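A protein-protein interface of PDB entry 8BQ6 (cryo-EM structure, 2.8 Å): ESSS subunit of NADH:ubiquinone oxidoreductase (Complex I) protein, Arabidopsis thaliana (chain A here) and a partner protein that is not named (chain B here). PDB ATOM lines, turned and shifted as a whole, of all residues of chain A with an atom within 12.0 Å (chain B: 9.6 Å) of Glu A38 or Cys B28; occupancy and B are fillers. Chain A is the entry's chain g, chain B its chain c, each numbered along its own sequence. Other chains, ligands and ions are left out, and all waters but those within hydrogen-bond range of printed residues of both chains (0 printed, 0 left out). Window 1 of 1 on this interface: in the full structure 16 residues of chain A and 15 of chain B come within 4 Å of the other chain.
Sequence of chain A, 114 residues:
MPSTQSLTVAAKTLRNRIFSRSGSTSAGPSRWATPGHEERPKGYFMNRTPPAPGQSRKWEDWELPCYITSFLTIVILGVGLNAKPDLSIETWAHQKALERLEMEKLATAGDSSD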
ATOM      1  N   SER A  30      14.150 -13.539 -27.124  1.00  0.00           N
ATOM      2  CA  SER A  30      14.070 -13.053 -25.752  1.00  0.00           C
ATOM      3  C   SER A  30      15.053 -11.912 -25.522  1.00  0.00           C
ATOM      4  O   SER A  30      14.863 -11.087 -24.628  1.00  0.00           O
ATOM      5  CB  SER A  30      14.346 -14.182 -24.761  1.00  0.00           C
ATOM      6  OG  SER A  30      15.688 -14.626 -24.862  1.00  0.00           O
ATOM      7  N   ARG A  31      16.110 -11.867 -26.335  1.00  0.00           N
ATOM      8  CA  ARG A  31      17.084 -10.791 -26.203  1.00  0.00           C
ATOM      9  C   ARG A  31      16.519  -9.435 -26.611  1.00  0.00           C
ATOM     10  O   ARG A  31      17.130  -8.412 -26.287  1.00  0.00           O
ATOM     11  CB  ARG A  31      18.342 -11.104 -27.021  1.00  0.00           C
ATOM     12  CG  ARG A  31      18.178 -10.925 -28.519  1.00  0.00           C
ATOM     13  CD  ARG A  31      19.446 -11.279 -29.279  1.00  0.00           C
ATOM     14  NE  ARG A  31      20.246 -10.108 -29.621  1.00  0.00           N
ATOM     15  CZ  ARG A  31      21.479 -10.162 -30.108  1.00  0.00           C
ATOM     16  NH1 ARG A  31      22.101 -11.316 -30.281  1.00  0.00           N
ATOM     17  NH2 ARG A  31      22.101  -9.033 -30.432  1.00  0.00           N
ATOM     18  N   TRP A  32      15.372  -9.398 -27.293  1.00  0.00           N
ATOM     19  CA  TRP A  32      14.756  -8.140 -27.696  1.00  0.00           C
ATOM     20  C   TRP A  32      13.504  -7.791 -26.901  1.00  0.00           C
ATOM     21  O   TRP A  32      13.068  -6.636 -26.943  1.00  0.00           O
ATOM     22  CB  TRP A  32      14.388  -8.168 -29.185  1.00  0.00           C
ATOM     23  CG  TRP A  32      15.429  -8.771 -30.072  1.00  0.00           C
ATOM     24  CD1 TRP A  32      15.419 -10.022 -30.606  1.00  0.00           C
ATOM     25  CD2 TRP A  32      16.631  -8.145 -30.536  1.00  0.00           C
ATOM     26  NE1 TRP A  32      16.540 -10.217 -31.369  1.00  0.00           N
ATOM     27  CE2 TRP A  32      17.301  -9.080 -31.345  1.00  0.00           C
ATOM     28  CE3 TRP A  32      17.205  -6.888 -30.343  1.00  0.00           C
ATOM     29  CZ2 TRP A  32      18.517  -8.799 -31.958  1.00  0.00           C
ATOM     30  CZ3 TRP A  32      18.406  -6.614 -30.955  1.00  0.00           C
ATOM     31  CH2 TRP A  32      19.052  -7.560 -31.753  1.00  0.00           C
ATOM     32  N   THR A  34      12.943  -9.035 -23.425  1.00  0.00           N
ATOM     33  CA  THR A  34      13.212  -8.989 -21.995  1.00  0.00           C
ATOM     34  C   THR A  34      14.306  -7.969 -21.737  1.00  0.00           C
ATOM     35  O   THR A  34      15.390  -8.078 -22.333  1.00  0.00           O
ATOM     36  CB  THR A  34      13.632 -10.357 -21.465  1.00  0.00           C
ATOM     37  OG1 THR A  34      14.613 -10.931 -22.339  1.00  0.00           O
ATOM     38  CG2 THR A  34      12.426 -11.281 -21.377  1.00  0.00           C
ATOM     39  N   PRO A  35      14.078  -6.968 -20.893  1.00  0.00           N
ATOM     40  CA  PRO A  35      15.119  -5.969 -20.633  1.00  0.00           C
ATOM     41  C   PRO A  35      16.341  -6.599 -19.984  1.00  0.00           C
ATOM     42  O   PRO A  35      16.319  -7.741 -19.520  1.00  0.00           O
ATOM     43  CB  PRO A  35      14.437  -4.979 -19.683  1.00  0.00           C
ATOM     44  CG  PRO A  35      13.352  -5.769 -19.030  1.00  0.00           C
ATOM     45  CD  PRO A  35      12.893  -6.780 -20.038  1.00  0.00           C
ATOM     46  N   GLY A  36      17.422  -5.827 -19.957  1.00  0.00           N
ATOM     47  CA  GLY A  36      18.670  -6.315 -19.414  1.00  0.00           C
ATOM     48  C   GLY A  36      18.648  -6.415 -17.900  1.00  0.00           C
ATOM     49  O   GLY A  36      17.658  -6.117 -17.230  1.00  0.00           O
ATOM     50  N   HIS A  37      19.784  -6.849 -17.352  1.00  0.00           N
ATOM     51  CA  HIS A  37      19.926  -7.039 -15.915  1.00  0.00           C
ATOM     52  C   HIS A  37      20.839  -6.019 -15.249  1.00  0.00           C
ATOM     53  O   HIS A  37      20.823  -5.917 -14.019  1.00  0.00           O
ATOM     54  CB  HIS A  37      20.467  -8.439 -15.614  1.00  0.00           C
ATOM     55  CG  HIS A  37      19.588  -9.539 -16.112  1.00  0.00           C
ATOM     56  ND1 HIS A  37      18.352  -9.808 -15.566  1.00  0.00           N
ATOM     57  CD2 HIS A  37      19.755 -10.429 -17.120  1.00  0.00           C
ATOM     58  CE1 HIS A  37      17.801 -10.824 -16.205  1.00  0.00           C
ATOM     59  NE2 HIS A  37      18.631 -11.217 -17.155  1.00  0.00           N
ATOM     60  N   GLU A  38      21.638  -5.273 -16.012  1.00  0.00           N
ATOM     61  CA  GLU A  38      22.534  -4.313 -15.381  1.00  0.00           C
ATOM     62  C   GLU A  38      21.759  -3.119 -14.844  1.00  0.00           C
ATOM     63  O   GLU A  38      21.511  -2.155 -15.574  1.00  0.00           O
ATOM     64  CB  GLU A  38      23.615  -3.833 -16.353  1.00  0.00           C
ATOM     65  CG  GLU A  38      24.177  -4.898 -17.267  1.00  0.00           C
ATOM     66  CD  GLU A  38      25.340  -4.389 -18.094  1.00  0.00           C
ATOM     67  OE1 GLU A  38      25.167  -3.412 -18.852  1.00  0.00           O
ATOM     68  OE2 GLU A  38      26.443  -4.960 -17.969  1.00  0.00           O
ATOM     69  N   GLU A  39      21.380  -3.173 -13.564  1.00  0.00           N
ATOM     70  CA  GLU A  39      20.726  -2.022 -12.950  1.00  0.00           C
ATOM     71  C   GLU A  39      21.636  -0.807 -12.995  1.00  0.00           C
ATOM     72  O   GLU A  39      21.183   0.312 -13.263  1.00  0.00           O
ATOM     73  CB  GLU A  39      20.319  -2.342 -11.513  1.00  0.00           C
ATOM     74  CG  GLU A  39      19.712  -3.720 -11.335  1.00  0.00           C
ATOM     75  CD  GLU A  39      20.751  -4.780 -11.028  1.00  0.00           C
ATOM     76  OE1 GLU A  39      21.917  -4.416 -10.770  1.00  0.00           O
ATOM     77  OE2 GLU A  39      20.405  -5.979 -11.054  1.00  0.00           O
ATOM     78  N   ARG A  40      22.924  -1.011 -12.753  1.00  0.00           N
ATOM     79  CA  ARG A  40      23.933   0.023 -12.881  1.00  0.00           C
ATOM     80  C   ARG A  40      25.119  -0.517 -13.664  1.00  0.00           C
ATOM     81  O   ARG A  40      25.423  -1.713 -13.596  1.00  0.00           O
ATOM     82  CB  ARG A  40      24.395   0.516 -11.504  1.00  0.00           C
ATOM     83  CG  ARG A  40      23.324   1.257 -10.712  1.00  0.00           C
ATOM     84  CD  ARG A  40      23.907   1.784  -9.418  1.00  0.00           C
ATOM     85  NE  ARG A  40      22.944   2.508  -8.599  1.00  0.00           N
ATOM     86  CZ  ARG A  40      23.228   3.025  -7.412  1.00  0.00           C
ATOM     87  NH1 ARG A  40      24.434   2.907  -6.880  1.00  0.00           N
ATOM     88  NH2 ARG A  40      22.286   3.688  -6.748  1.00  0.00           N
ATOM     89  N   PRO A  41      25.805   0.338 -14.416  1.00  0.00           N
ATOM     90  CA  PRO A  41      26.919  -0.132 -15.246  1.00  0.00           C
ATOM     91  C   PRO A  41      28.056  -0.697 -14.408  1.00  0.00           C
ATOM     92  O   PRO A  41      28.261  -0.342 -13.246  1.00  0.00           O
ATOM     93  CB  PRO A  41      27.354   1.127 -15.998  1.00  0.00           C
ATOM     94  CG  PRO A  41      26.179   2.033 -15.949  1.00  0.00           C
ATOM     95  CD  PRO A  41      25.511   1.761 -14.642  1.00  0.00           C
ATOM     96  N   LYS A  42      28.796  -1.616 -15.027  1.00  0.00           N
ATOM     97  CA  LYS A  42      29.939  -2.239 -14.378  1.00  0.00           C
ATOM     98  C   LYS A  42      31.096  -1.252 -14.272  1.00  0.00           C
ATOM     99  O   LYS A  42      31.408  -0.531 -15.224  1.00  0.00           O
ATOM    100  CB  LYS A  42      30.366  -3.498 -15.139  1.00  0.00           C
ATOM    101  CG  LYS A  42      30.466  -3.335 -16.647  1.00  0.00           C
ATOM    102  CD  LYS A  42      31.300  -4.444 -17.274  1.00  0.00           C
ATOM    103  CE  LYS A  42      30.506  -5.726 -17.492  1.00  0.00           C
ATOM    104  NZ  LYS A  42      29.569  -5.608 -18.640  1.00  0.00           N
ATOM    105  N   GLY A  43      31.713  -1.208 -13.093  1.00  0.00           N
ATOM    106  CA  GLY A  43      32.806  -0.292 -12.843  1.00  0.00           C
ATOM    107  C   GLY A  43      32.328   1.116 -12.550  1.00  0.00           C
ATOM    108  O   GLY A  43      31.135   1.419 -12.505  1.00  0.00           O
ATOM    109  N   TYR A  44      33.300   1.999 -12.341  1.00  0.00           N
ATOM    110  CA  TYR A  44      33.031   3.403 -12.082  1.00  0.00           C
ATOM    111  C   TYR A  44      33.873   4.259 -13.010  1.00  0.00           C
ATOM    112  O   TYR A  44      35.033   3.941 -13.285  1.00  0.00           O
ATOM    113  CB  TYR A  44      33.311   3.765 -10.627  1.00  0.00           C
ATOM    114  CG  TYR A  44      32.278   3.190  -9.705  1.00  0.00           C
ATOM    115  CD1 TYR A  44      30.929   3.396  -9.943  1.00  0.00           C
ATOM    116  CD2 TYR A  44      32.643   2.412  -8.619  1.00  0.00           C
ATOM    117  CE1 TYR A  44      29.975   2.861  -9.121  1.00  0.00           C
ATOM    118  CE2 TYR A  44      31.693   1.868  -7.788  1.00  0.00           C
ATOM    119  CZ  TYR A  44      30.360   2.099  -8.043  1.00  0.00           C
ATOM    120  OH  TYR A  44      29.397   1.566  -7.223  1.00  0.00           O
ATOM    121  N   ARG B  16      35.838  -8.361 -14.183  1.00  0.00           N
ATOM    122  CA  ARG B  16      35.432  -7.441 -15.236  1.00  0.00           C
ATOM    123  C   ARG B  16      34.171  -6.670 -14.874  1.00  0.00           C
ATOM    124  O   ARG B  16      33.880  -5.651 -15.507  1.00  0.00           O
ATOM    125  CB  ARG B  16      35.252  -8.205 -16.543  1.00  0.00           C
ATOM    126  CG  ARG B  16      36.378  -9.190 -16.787  1.00  0.00           C
ATOM    127  CD  ARG B  16      36.816  -9.182 -18.230  1.00  0.00           C
ATOM    128  NE  ARG B  16      35.847  -9.854 -19.082  1.00  0.00           N
ATOM    129  CZ  ARG B  16      35.918 -11.129 -19.434  1.00  0.00           C
ATOM    130  NH1 ARG B  16      36.936 -11.889 -19.072  1.00  0.00           N
ATOM    131  NH2 ARG B  16      34.946 -11.653 -20.174  1.00  0.00           N
ATOM    132  N   ALA B  17      33.433  -7.118 -13.859  1.00  0.00           N
ATOM    133  CA  ALA B  17      32.280  -6.370 -13.379  1.00  0.00           C
ATOM    134  C   ALA B  17      32.671  -5.098 -12.636  1.00  0.00           C
ATOM    135  O   ALA B  17      31.804  -4.250 -12.402  1.00  0.00           O
ATOM    136  CB  ALA B  17      31.427  -7.256 -12.473  1.00  0.00           C
ATOM    137  N   LYS B  18      33.936  -4.953 -12.252  1.00  0.00           N
ATOM    138  CA  LYS B  18      34.431  -3.750 -11.596  1.00  0.00           C
ATOM    139  C   LYS B  18      35.215  -2.850 -12.535  1.00  0.00           C
ATOM    140  O   LYS B  18      35.847  -1.893 -12.078  1.00  0.00           O
ATOM    141  CB  LYS B  18      35.311  -4.120 -10.406  1.00  0.00           C
ATOM    142  CG  LYS B  18      34.721  -5.169  -9.497  1.00  0.00           C
ATOM    143  CD  LYS B  18      35.700  -5.542  -8.400  1.00  0.00           C
ATOM    144  CE  LYS B  18      36.500  -4.336  -7.929  1.00  0.00           C
ATOM    145  NZ  LYS B  18      35.641  -3.301  -7.301  1.00  0.00           N
ATOM    146  N   VAL B  19      35.201  -3.138 -13.831  1.00  0.00           N
ATOM    147  CA  VAL B  19      36.011  -2.423 -14.804  1.00  0.00           C
ATOM    148  C   VAL B  19      35.077  -1.613 -15.691  1.00  0.00           C
ATOM    149  O   VAL B  19      34.185  -2.170 -16.341  1.00  0.00           O
ATOM    150  CB  VAL B  19      36.874  -3.387 -15.631  1.00  0.00           C
ATOM    151  CG1 VAL B  19      37.404  -2.698 -16.868  1.00  0.00           C
ATOM    152  CG2 VAL B  19      38.012  -3.928 -14.780  1.00  0.00           C
ATOM    153  N   SER B  21      34.228   0.677 -18.945  1.00  0.00           N
ATOM    154  CA  SER B  21      34.652   0.825 -20.330  1.00  0.00           C
ATOM    155  C   SER B  21      33.543   1.497 -21.126  1.00  0.00           C
ATOM    156  O   SER B  21      32.359   1.376 -20.808  1.00  0.00           O
ATOM    157  CB  SER B  21      35.009  -0.523 -20.967  1.00  0.00           C
ATOM    158  OG  SER B  21      33.940  -1.440 -20.841  1.00  0.00           O
ATOM    159  N   MET B  22      33.949   2.198 -22.188  1.00  0.00           N
ATOM    160  CA  MET B  22      32.988   2.949 -22.991  1.00  0.00           C
ATOM    161  C   MET B  22      32.046   2.025 -23.756  1.00  0.00           C
ATOM    162  O   MET B  22      30.856   2.331 -23.898  1.00  0.00           O
ATOM    163  CB  MET B  22      33.725   3.882 -23.951  1.00  0.00           C
ATOM    164  CG  MET B  22      34.241   5.156 -23.300  1.00  0.00           C
ATOM    165  SD  MET B  22      35.098   6.245 -24.451  1.00  0.00           S
ATOM    166  CE  MET B  22      35.847   5.045 -25.540  1.00  0.00           C
ATOM    167  N   THR B  23      32.552   0.898 -24.262  1.00  0.00           N
ATOM    168  CA  THR B  23      31.716  -0.028 -25.019  1.00  0.00           C
ATOM    169  C   THR B  23      30.952  -1.007 -24.139  1.00  0.00           C
ATOM    170  O   THR B  23      30.136  -1.773 -24.660  1.00  0.00           O
ATOM    171  CB  THR B  23      32.554  -0.816 -26.028  1.00  0.00           C
ATOM    172  OG1 THR B  23      33.695  -1.373 -25.369  1.00  0.00           O
ATOM    173  CG2 THR B  23      33.019   0.073 -27.165  1.00  0.00           C
ATOM    174  N   GLY B  24      31.193  -1.012 -22.831  1.00  0.00           N
ATOM    175  CA  GLY B  24      30.370  -1.759 -21.907  1.00  0.00           C
ATOM    176  C   GLY B  24      30.951  -3.064 -21.410  1.00  0.00           C
ATOM    177  O   GLY B  24      30.358  -3.680 -20.517  1.00  0.00           O
ATOM    178  N   GLY B  25      32.082  -3.507 -21.948  1.00  0.00           N
ATOM    179  CA  GLY B  25      32.684  -4.740 -21.505  1.00  0.00           C
ATOM    180  C   GLY B  25      31.927  -5.950 -22.008  1.00  0.00           C
ATOM    181  O   GLY B  25      31.173  -5.880 -22.981  1.00  0.00           O
ATOM    182  N   PRO B  26      32.100  -7.087 -21.341  1.00  0.00           N
ATOM    183  CA  PRO B  26      31.539  -8.339 -21.855  1.00  0.00           C
ATOM    184  C   PRO B  26      30.113  -8.584 -21.386  1.00  0.00           C
ATOM    185  O   PRO B  26      29.787  -8.427 -20.205  1.00  0.00           O
ATOM    186  CB  PRO B  26      32.491  -9.400 -21.295  1.00  0.00           C
ATOM    187  CG  PRO B  26      33.108  -8.764 -20.083  1.00  0.00           C
ATOM    188  CD  PRO B  26      32.816  -7.292 -20.074  1.00  0.00           C
ATOM    189  N   ASN B  27      29.268  -8.998 -22.333  1.00  0.00           N
ATOM    190  CA  ASN B  27      27.863  -9.317 -22.074  1.00  0.00           C
ATOM    191  C   ASN B  27      27.132  -8.126 -21.462  1.00  0.00           C
ATOM    192  O   ASN B  27      26.462  -8.236 -20.434  1.00  0.00           O
ATOM    193  CB  ASN B  27      27.729 -10.549 -21.179  1.00  0.00           C
ATOM    194  CG  ASN B  27      28.374 -11.769 -21.777  1.00  0.00           C
ATOM    195  OD1 ASN B  27      28.047 -12.174 -22.892  1.00  0.00           O
ATOM    196  ND2 ASN B  27      29.298 -12.371 -21.039  1.00  0.00           N
ATOM    197  N   CYS B  28      27.272  -6.973 -22.106  1.00  0.00           N
ATOM    198  CA  CYS B  28      26.636  -5.754 -21.632  1.00  0.00           C
ATOM    199  C   CYS B  28      25.146  -5.820 -21.949  1.00  0.00           C
ATOM    200  O   CYS B  28      24.756  -5.917 -23.118  1.00  0.00           O
ATOM    201  CB  CYS B  28      27.295  -4.538 -22.279  1.00  0.00           C
ATOM    202  SG  CYS B  28      26.795  -2.935 -21.635  1.00  0.00           S
ATOM    203  N   ARG B  29      24.322  -5.800 -20.905  1.00  0.00           N
ATOM    204  CA  ARG B  29      22.868  -5.892 -21.023  1.00  0.00           C
ATOM    205  C   ARG B  29      22.232  -4.798 -20.180  1.00  0.00           C
ATOM    206  O   ARG B  29      21.655  -5.074 -19.122  1.00  0.00           O
ATOM    207  CB  ARG B  29      22.376  -7.263 -20.565  1.00  0.00           C
ATOM    208  CG  ARG B  29      22.874  -8.424 -21.389  1.00  0.00           C
ATOM    209  CD  ARG B  29      21.925  -8.705 -22.518  1.00  0.00           C
ATOM    210  NE  ARG B  29      20.540  -8.649 -22.069  1.00  0.00           N
ATOM    211  CZ  ARG B  29      19.502  -9.005 -22.812  1.00  0.00           C
ATOM    212  NH1 ARG B  29      19.661  -9.481 -24.036  1.00  0.00           N
ATOM    213  NH2 ARG B  29      18.276  -8.880 -22.315  1.00  0.00           N
ATOM    214  N   PRO B  30      22.342  -3.539 -20.598  1.00  0.00           N
ATOM    215  CA  PRO B  30      21.714  -2.466 -19.822  1.00  0.00           C
ATOM    216  C   PRO B  30      20.204  -2.651 -19.765  1.00  0.00           C
ATOM    217  O   PRO B  30      19.565  -3.017 -20.753  1.00  0.00           O
ATOM    218  CB  PRO B  30      22.112  -1.194 -20.580  1.00  0.00           C
ATOM    219  CG  PRO B  30      22.510  -1.650 -21.927  1.00  0.00           C
ATOM    220  CD  PRO B  30      23.053  -3.028 -21.778  1.00  0.00           C
ATOM    221  N   LYS B  31      19.639  -2.400 -18.581  1.00  0.00           N
ATOM    222  CA  LYS B  31      18.228  -2.696 -18.348  1.00  0.00           C
ATOM    223  C   LYS B  31      17.325  -1.827 -19.211  1.00  0.00           C
ATOM    224  O   LYS B  31      16.329  -2.307 -19.763  1.00  0.00           O
ATOM    225  CB  LYS B  31      17.902  -2.519 -16.863  1.00  0.00           C
ATOM    226  CG  LYS B  31      16.423  -2.378 -16.547  1.00  0.00           C
ATOM    227  CD  LYS B  31      16.163  -2.336 -15.042  1.00  0.00           C
ATOM    228  CE  LYS B  31      17.376  -1.841 -14.260  1.00  0.00           C
ATOM    229  NZ  LYS B  31      17.151  -1.841 -12.787  1.00  0.00           N
ATOM    230  N   HIS B  32      17.667  -0.552 -19.356  1.00  0.00           N
ATOM    231  CA  HIS B  32      16.889   0.399 -20.145  1.00  0.00           C
ATOM    232  C   HIS B  32      17.470   0.565 -21.539  1.00  0.00           C
ATOM    233  O   HIS B  32      17.486   1.670 -22.087  1.00  0.00           O
ATOM    234  CB  HIS B  32      16.810   1.746 -19.432  1.00  0.00           C
ATOM    235  CG  HIS B  32      16.407   1.656 -17.991  1.00  0.00           C
ATOM    236  ND1 HIS B  32      17.106   0.917 -17.061  1.00  0.00           N
ATOM    237  CD2 HIS B  32      15.391   2.242 -17.316  1.00  0.00           C
ATOM    238  CE1 HIS B  32      16.525   1.034 -15.880  1.00  0.00           C
ATOM    239  NE2 HIS B  32      15.483   1.834 -16.008  1.00  0.00           N
ATOM    240  N   TRP B  33      17.970  -0.524 -22.132  1.00  0.00           N
ATOM    241  CA  TRP B  33      18.683  -0.405 -23.398  1.00  0.00           C
ATOM    242  C   TRP B  33      17.771   0.029 -24.537  1.00  0.00           C
ATOM    243  O   TRP B  33      18.262   0.527 -25.554  1.00  0.00           O
ATOM    244  CB  TRP B  33      19.391  -1.721 -23.744  1.00  0.00           C
ATOM    245  CG  TRP B  33      18.505  -2.845 -24.196  1.00  0.00           C
ATOM    246  CD1 TRP B  33      18.020  -3.859 -23.427  1.00  0.00           C
ATOM    247  CD2 TRP B  33      18.025  -3.085 -25.525  1.00  0.00           C
ATOM    248  NE1 TRP B  33      17.260  -4.710 -24.189  1.00  0.00           N
ATOM    249  CE2 TRP B  33      17.245  -4.256 -25.481  1.00  0.00           C
ATOM    250  CE3 TRP B  33      18.172  -2.421 -26.747  1.00  0.00           C
ATOM    251  CZ2 TRP B  33      16.614  -4.777 -26.607  1.00  0.00           C
ATOM    252  CZ3 TRP B  33      17.543  -2.940 -27.864  1.00  0.00           C
ATOM    253  CH2 TRP B  33      16.776  -4.106 -27.787  1.00  0.00           C
ATOM    254  N   ARG B  35      15.105   2.366 -24.385  1.00  0.00           N
ATOM    255  CA  ARG B  35      14.936   3.814 -24.374  1.00  0.00           C
ATOM    256  C   ARG B  35      16.250   4.516 -24.690  1.00  0.00           C
ATOM    257  O   ARG B  35      16.254   5.628 -25.230  1.00  0.00           O
ATOM    258  CB  ARG B  35      14.389   4.282 -23.024  1.00  0.00           C
ATOM    259  CG  ARG B  35      15.335   4.052 -21.846  1.00  0.00           C
ATOM    260  CD  ARG B  35      14.724   4.489 -20.528  1.00  0.00           C
ATOM    261  NE  ARG B  35      15.640   4.289 -19.411  1.00  0.00           N
ATOM    262  CZ  ARG B  35      16.538   5.177 -19.007  1.00  0.00           C
ATOM    263  NH1 ARG B  35      16.681   6.342 -19.617  1.00  0.00           N
ATOM    264  NH2 ARG B  35      17.317   4.887 -17.969  1.00  0.00           N
ATOM    265  N   ASN B  36      17.376   3.891 -24.345  1.00  0.00           N
ATOM    266  CA  ASN B  36      18.667   4.464 -24.708  1.00  0.00           C
ATOM    267  C   ASN B  36      18.935   4.290 -26.193  1.00  0.00           C
ATOM    268  O   ASN B  36      19.523   5.172 -26.830  1.00  0.00           O
ATOM    269  CB  ASN B  36      19.782   3.828 -23.885  1.00  0.00           C
ATOM    270  CG  ASN B  36      19.602   4.046 -22.406  1.00  0.00           C
ATOM    271  OD1 ASN B  36      18.881   4.947 -21.986  1.00  0.00           O
ATOM    272  ND2 ASN B  36      20.256   3.220 -21.603  1.00  0.00           N
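O of Ala B17 lies within hydrogen-bond range of N of Gly A43 (3.1 Å).
The backbone carbonyl oxygen (O) of Gly B24 sits at hydrogen-bond distance from the side-chain amino group (NZ) of Lys A42, at 2.8 Å.
The backbone carbonyl oxygen (O) of Pro B26 lies within hydrogen-bond range of the side-chain amino group (NZ) of Lys A42 (3.2 Å).
The side-chain carboxylate of Glu A38 lies within hydrogen-bond range of the side-chain sulfur of Cys B28 (3.3 Å).
The guanidinium group (NH2) of Arg B29 lies within hydrogen-bond range of the backbone carbonyl oxygen (O) of Thr A34 (3.0 Å).
The backbone carbonyl oxygen (O) of Arg B29 lies within hydrogen-bond range of the backbone NH (N) of His A37 (3.1 Å).
O of Arg B29 sits at hydrogen-bond distance from N of Glu A38, at 3.1 Å.
The backbone nitrogen (N) of Pro B30 lies close to the side-chain carboxylate (OE1) of Glu A38, 3.3 Å away.
The backbone carbonyl oxygen (O) of Lys A42 lies close to the backbone carbonyl oxygen (O) of Val B19.
OG of Ser B21 sits at hydrogen-bond distance from N of Gly B24, 3.4 Å away.
The side-chain carboxylate (OE2) of Glu A38 lies within salt-bridge range of the side-chain amino group (NZ) of Lys A42, 3.3 Å away.
Among the printed residues, pairs that only touch across the chains: Arg A31 with Arg B29 (3.6 Å), Arg A31 with Trp B33 (3.7 Å), Trp A32 with Trp B33 (3.8 Å), Pro A35 with Arg B29 (3.6 Å), Pro A35 with Lys B31 (3.3 Å), Gly A36 with Arg B29 (3.2 Å), Gly A36 with Pro B30 (3.6 Å), Gly A36 with Lys B31 (3.6 Å), Glu A38 with Lys B31 (3.6 Å), Glu A39 with Lys B31 (3.5 Å), Lys A42 with Arg B16 (3.4 Å), Lys A42 with Ala B17 (3.2 Å), Gly A43 with Lys B18 (3.5 Å) and Gly A43 with Val B19 (3.8 Å).
Ser A30 touches none of the printed residues of chain B.
Of the printed residues of chain B, Gly A36 touches Arg B29 (3.2 Å), Pro B30 (3.6 Å) and Lys B31 (3.6 Å).
Glu A38 touches just these residues of chain B: Cys B28, Arg B29, Pro B30 and Lys B31.
Of the printed residues of chain B, Lys A42 touches Arg B16 (3.4 Å), Ala B17 (3.2 Å), Val B19 (3.4 Å), Gly B24 (2.8 Å) and Pro B26 (3.2 Å).
Printed residues of chain A within 4 Å of Arg B16: Lys A42.
Of the printed residues of chain A, Ala B17 touches Lys A42 and Gly A43.
Pro B26 touches just one residue of chain A: Lys A42 (3.2 Å).
Arg B29 touches just these residues of chain A: Arg A31 (3.6 Å), Thr A34 (3.0 Å), Pro A35 (3.6 Å), Gly A36 (3.2 Å), His A37 (3.1 Å) and Glu A38 (3.1 Å).
Of chain A, only Gly A36 (3.6 Å) and Glu A38 (3.3 Å) come within 4 Å of Pro B30.
Lys B31 touches just these residues of chain A: Pro A35 (3.3 Å), Gly A36 (3.6 Å), Glu A38 (3.6 Å) and Glu A39 (3.5 Å).
The nearest residue of chain B that does not touch Glu A38 is Asn B27 (4.1 Å).
The nearest printed residue of chain B that does not touch Lys A42 is Gly B25 (4.1 Å).
Among the printed residues, 23 pairs touch across the chains.
Among the printed residues, no Asp or Glu carboxylate lies within 4 Å of a Lys or Arg side-chain nitrogen of the other chain.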
